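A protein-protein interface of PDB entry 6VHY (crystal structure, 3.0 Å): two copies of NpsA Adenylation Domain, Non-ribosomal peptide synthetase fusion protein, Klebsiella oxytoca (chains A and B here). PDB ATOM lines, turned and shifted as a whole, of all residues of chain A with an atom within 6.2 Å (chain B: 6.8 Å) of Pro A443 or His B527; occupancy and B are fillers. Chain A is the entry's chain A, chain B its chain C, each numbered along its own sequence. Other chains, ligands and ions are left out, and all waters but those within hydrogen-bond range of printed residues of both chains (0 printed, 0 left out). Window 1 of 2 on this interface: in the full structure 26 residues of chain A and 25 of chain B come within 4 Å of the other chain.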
ATOM      1  N   ASN A 278      11.181   0.571 -23.133  1.00  0.00           N
ATOM      2  CA  ASN A 278      10.059   0.898 -23.994  1.00  0.00           C
ATOM      3  C   ASN A 278       9.015   1.670 -23.200  1.00  0.00           C
ATOM      4  O   ASN A 278       8.638   1.246 -22.103  1.00  0.00           O
ATOM      5  CB  ASN A 278       9.450  -0.373 -24.578  1.00  0.00           C
ATOM      6  CG  ASN A 278       8.547  -0.100 -25.759  1.00  0.00           C
ATOM      7  OD1 ASN A 278       7.524   0.569 -25.639  1.00  0.00           O
ATOM      8  ND2 ASN A 278       8.932  -0.611 -26.917  1.00  0.00           N
ATOM      9  N   GLU A 441      18.410  -6.049 -33.736  1.00  0.00           N
ATOM     10  CA  GLU A 441      17.193  -5.535 -33.119  1.00  0.00           C
ATOM     11  C   GLU A 441      16.250  -6.688 -32.801  1.00  0.00           C
ATOM     12  O   GLU A 441      15.858  -7.441 -33.699  1.00  0.00           O
ATOM     13  CB  GLU A 441      16.515  -4.525 -34.041  1.00  0.00           C
ATOM     14  N   THR A 442      15.887  -6.826 -31.534  1.00  0.00           N
ATOM     15  CA  THR A 442      14.981  -7.862 -31.075  1.00  0.00           C
ATOM     16  C   THR A 442      13.718  -7.226 -30.513  1.00  0.00           C
ATOM     17  O   THR A 442      13.712  -6.041 -30.161  1.00  0.00           O
ATOM     18  CB  THR A 442      15.638  -8.734 -29.997  1.00  0.00           C
ATOM     19  OG1 THR A 442      15.782  -7.979 -28.790  1.00  0.00           O
ATOM     20  CG2 THR A 442      17.001  -9.194 -30.460  1.00  0.00           C
ATOM     21  N   PRO A 443      12.624  -7.985 -30.415  1.00  0.00           N
ATOM     22  CA  PRO A 443      11.437  -7.453 -29.734  1.00  0.00           C
ATOM     23  C   PRO A 443      11.712  -7.017 -28.310  1.00  0.00           C
ATOM     24  O   PRO A 443      11.075  -6.071 -27.830  1.00  0.00           O
ATOM     25  CB  PRO A 443      10.451  -8.631 -29.784  1.00  0.00           C
ATOM     26  CG  PRO A 443      11.280  -9.822 -30.150  1.00  0.00           C
ATOM     27  CD  PRO A 443      12.340  -9.286 -31.036  1.00  0.00           C
ATOM     28  N   ASP A 444      12.640  -7.666 -27.621  1.00  0.00           N
ATOM     29  CA  ASP A 444      12.929  -7.376 -26.227  1.00  0.00           C
ATOM     30  C   ASP A 444      14.161  -6.453 -26.174  1.00  0.00           C
ATOM     31  O   ASP A 444      14.138  -5.425 -26.853  1.00  0.00           O
ATOM     32  CB  ASP A 444      13.070  -8.685 -25.459  1.00  0.00           C
ATOM     33  CG  ASP A 444      11.819  -9.517 -25.513  1.00  0.00           C
ATOM     34  OD1 ASP A 444      11.930 -10.759 -25.477  1.00  0.00           O
ATOM     35  OD2 ASP A 444      10.723  -8.929 -25.591  1.00  0.00           O
ATOM     36  N   GLU A 445      15.200  -6.777 -25.440  1.00  0.00           N
ATOM     37  CA  GLU A 445      16.417  -5.990 -25.477  1.00  0.00           C
ATOM     38  C   GLU A 445      17.277  -6.440 -26.655  1.00  0.00           C
ATOM     39  O   GLU A 445      17.213  -7.600 -27.067  1.00  0.00           O
ATOM     40  CB  GLU A 445      17.191  -6.149 -24.171  1.00  0.00           C
ATOM     41  CG  GLU A 445      16.528  -5.507 -22.960  1.00  0.00           C
ATOM     42  CD  GLU A 445      15.388  -6.332 -22.408  1.00  0.00           C
ATOM     43  OE1 GLU A 445      15.427  -7.569 -22.554  1.00  0.00           O
ATOM     44  OE2 GLU A 445      14.450  -5.749 -21.829  1.00  0.00           O
ATOM     45  N   ILE B 521       5.003 -22.112 -22.751  1.00  0.00           N
ATOM     46  CA  ILE B 521       5.480 -20.926 -22.042  1.00  0.00           C
ATOM     47  C   ILE B 521       6.889 -20.551 -22.487  1.00  0.00           C
ATOM     48  O   ILE B 521       7.176 -19.384 -22.779  1.00  0.00           O
ATOM     49  CB  ILE B 521       5.410 -21.165 -20.523  1.00  0.00           C
ATOM     50  CG1 ILE B 521       3.954 -21.171 -20.051  1.00  0.00           C
ATOM     51  CG2 ILE B 521       6.237 -20.150 -19.775  1.00  0.00           C
ATOM     52  CD1 ILE B 521       3.788 -21.525 -18.597  1.00  0.00           C
ATOM     53  N   TRP B 522       7.784 -21.533 -22.570  1.00  0.00           N
ATOM     54  CA  TRP B 522       9.160 -21.248 -22.972  1.00  0.00           C
ATOM     55  C   TRP B 522       9.245 -20.811 -24.427  1.00  0.00           C
ATOM     56  O   TRP B 522      10.080 -19.971 -24.779  1.00  0.00           O
ATOM     57  CB  TRP B 522      10.046 -22.467 -22.722  1.00  0.00           C
ATOM     58  CG  TRP B 522      11.486 -22.274 -23.115  1.00  0.00           C
ATOM     59  CD1 TRP B 522      12.126 -22.866 -24.163  1.00  0.00           C
ATOM     60  CD2 TRP B 522      12.448 -21.407 -22.501  1.00  0.00           C
ATOM     61  NE1 TRP B 522      13.429 -22.444 -24.227  1.00  0.00           N
ATOM     62  CE2 TRP B 522      13.652 -21.545 -23.219  1.00  0.00           C
ATOM     63  CE3 TRP B 522      12.411 -20.531 -21.414  1.00  0.00           C
ATOM     64  CZ2 TRP B 522      14.805 -20.844 -22.883  1.00  0.00           C
ATOM     65  CZ3 TRP B 522      13.557 -19.842 -21.079  1.00  0.00           C
ATOM     66  CH2 TRP B 522      14.737 -20.000 -21.811  1.00  0.00           C
ATOM     67  N   GLN B 523       8.398 -21.369 -25.288  1.00  0.00           N
ATOM     68  CA  GLN B 523       8.403 -20.953 -26.684  1.00  0.00           C
ATOM     69  C   GLN B 523       7.909 -19.524 -26.855  1.00  0.00           C
ATOM     70  O   GLN B 523       8.324 -18.841 -27.797  1.00  0.00           O
ATOM     71  CB  GLN B 523       7.548 -21.911 -27.512  1.00  0.00           C
ATOM     72  N   ALA B 524       7.043 -19.049 -25.961  1.00  0.00           N
ATOM     73  CA  ALA B 524       6.643 -17.647 -26.005  1.00  0.00           C
ATOM     74  C   ALA B 524       7.744 -16.731 -25.487  1.00  0.00           C
ATOM     75  O   ALA B 524       7.926 -15.620 -25.999  1.00  0.00           O
ATOM     76  CB  ALA B 524       5.358 -17.442 -25.206  1.00  0.00           C
ATOM     77  N   ILE B 525       8.494 -17.178 -24.479  1.00  0.00           N
ATOM     78  CA  ILE B 525       9.580 -16.367 -23.940  1.00  0.00           C
ATOM     79  C   ILE B 525      10.680 -16.179 -24.975  1.00  0.00           C
ATOM     80  O   ILE B 525      11.248 -15.089 -25.108  1.00  0.00           O
ATOM     81  CB  ILE B 525      10.123 -17.010 -22.653  1.00  0.00           C
ATOM     82  CG1 ILE B 525       9.053 -16.977 -21.572  1.00  0.00           C
ATOM     83  CG2 ILE B 525      11.373 -16.301 -22.182  1.00  0.00           C
ATOM     84  CD1 ILE B 525       9.378 -17.846 -20.410  1.00  0.00           C
ATOM     85  N   ILE B 526      10.994 -17.233 -25.733  1.00  0.00           N
ATOM     86  CA  ILE B 526      11.986 -17.122 -26.793  1.00  0.00           C
ATOM     87  C   ILE B 526      11.350 -16.817 -28.136  1.00  0.00           C
ATOM     88  O   ILE B 526      12.065 -16.744 -29.146  1.00  0.00           O
ATOM     89  CB  ILE B 526      12.833 -18.408 -26.892  1.00  0.00           C
ATOM     90  N   HIS B 527      10.023 -16.665 -28.184  1.00  0.00           N
ATOM     91  CA  HIS B 527       9.283 -16.309 -29.392  1.00  0.00           C
ATOM     92  C   HIS B 527       9.279 -17.430 -30.425  1.00  0.00           C
ATOM     93  O   HIS B 527       8.275 -17.627 -31.120  1.00  0.00           O
ATOM     94  CB  HIS B 527       9.821 -15.010 -29.998  1.00  0.00           C
ATOM     95  CG  HIS B 527      10.088 -13.943 -28.984  1.00  0.00           C
ATOM     96  ND1 HIS B 527       9.356 -13.823 -27.822  1.00  0.00           N
ATOM     97  CD2 HIS B 527      11.005 -12.947 -28.955  1.00  0.00           C
ATOM     98  CE1 HIS B 527       9.810 -12.799 -27.122  1.00  0.00           C
ATOM     99  NE2 HIS B 527      10.811 -12.252 -27.788  1.00  0.00           N
ATOM    100  N   SER B 528      10.380 -18.169 -30.545  1.00  0.00           N
ATOM    101  CA  SER B 528      10.483 -19.207 -31.567  1.00  0.00           C
ATOM    102  C   SER B 528       9.724 -20.433 -31.081  1.00  0.00           C
ATOM    103  O   SER B 528      10.272 -21.321 -30.428  1.00  0.00           O
ATOM    104  CB  SER B 528      11.942 -19.530 -31.857  1.00  0.00           C
ATOM    105  N   GLU B 529       8.430 -20.470 -31.404  1.00  0.00           N
ATOM    106  CA  GLU B 529       7.603 -21.620 -31.060  1.00  0.00           C
ATOM    107  C   GLU B 529       8.068 -22.878 -31.774  1.00  0.00           C
ATOM    108  O   GLU B 529       7.934 -23.984 -31.240  1.00  0.00           O
ATOM    109  CB  GLU B 529       6.140 -21.332 -31.392  1.00  0.00           C
ATOM    110  N   ALA B 530       8.622 -22.729 -32.973  1.00  0.00           N
ATOM    111  CA  ALA B 530       8.978 -23.868 -33.807  1.00  0.00           C
ATOM    112  C   ALA B 530      10.429 -24.291 -33.642  1.00  0.00           C
ATOM    113  O   ALA B 530      10.743 -25.474 -33.813  1.00  0.00           O
ATOM    114  CB  ALA B 530       8.693 -23.551 -35.277  1.00  0.00           C
ATOM    115  N   HIS B 546      15.445 -14.674 -19.729  1.00  0.00           N
ATOM    116  CA  HIS B 546      14.495 -15.678 -20.194  1.00  0.00           C
ATOM    117  C   HIS B 546      14.227 -16.737 -19.133  1.00  0.00           C
ATOM    118  O   HIS B 546      13.084 -17.175 -18.966  1.00  0.00           O
ATOM    119  CB  HIS B 546      15.007 -16.332 -21.473  1.00  0.00           C
ATOM    120  CG  HIS B 546      15.150 -15.385 -22.622  1.00  0.00           C
ATOM    121  ND1 HIS B 546      15.966 -14.276 -22.577  1.00  0.00           N
ATOM    122  CD2 HIS B 546      14.578 -15.379 -23.850  1.00  0.00           C
ATOM    123  CE1 HIS B 546      15.896 -13.631 -23.726  1.00  0.00           C
ATOM    124  NE2 HIS B 546      15.059 -14.278 -24.516  1.00  0.00           N
ATOM    125  N   LYS B 549      12.065 -15.231 -16.245  1.00  0.00           N
ATOM    126  CA  LYS B 549      10.675 -15.113 -16.676  1.00  0.00           C
ATOM    127  C   LYS B 549       9.962 -16.462 -16.655  1.00  0.00           C
ATOM    128  O   LYS B 549       8.798 -16.550 -16.248  1.00  0.00           O
ATOM    129  CB  LYS B 549      10.642 -14.485 -18.069  1.00  0.00           C
ATOM    130  CG  LYS B 549       9.283 -14.021 -18.579  1.00  0.00           C
ATOM    131  CD  LYS B 549       9.457 -13.362 -19.947  1.00  0.00           C
ATOM    132  CE  LYS B 549       8.141 -13.030 -20.624  1.00  0.00           C
ATOM    133  NZ  LYS B 549       7.015 -13.853 -20.146  1.00  0.00           N
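Printed residues of chain A that touch a printed residue of chain B: Pro A443 and Asp A444. Hydrophobic or aromatic side chains of chain A within 4 Å of the printed part of chain B: Pro A443. Of the 12 printed residues of chain B, 1 touches a printed residue of chain A. Printed residues of chain B that touch a printed residue of chain A: His B527. Hydrophobic or aromatic side chains of chain B within 4 Å of the printed part of chain A: His B527. Among the printed residues, no Asp or Glu carboxylate lies within 4 Å of a Lys or Arg side-chain nitrogen of the other chain.
OG1 of Thr A442 lies close to N of Asp A444. O of Ala B524 is in hydrogen-bond range of ND1 of His B527, 2.9 Å away.
OD1 of Asp A444 is in hydrogen-bond range of NE2 of His B527, 3.0 Å away.
Of chain B, only His B527 comes within 4 Å of Pro A443. His B527 touches just these residues of chain A: Pro A443 (3.4 Å) and Asp A444 (3.0 Å). Of the printed residues of chain B, Asp A444 touches His B527 (3.0 Å). Ile B521 touches none of the printed residues of chain A. The nearest printed residue of chain B that does not touch Pro A443 is Ile B526 (7.0 Å). The nearest printed residue of chain A that does not touch His B527 is Thr A442 (6.3 Å). The nearest printed residue of chain B that does not touch Asp A444 is Ile B525 (4.4 Å).
No position is printed for both chains.
CG of Pro A443 touches CD2 of His B527, 3.4 Å away.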
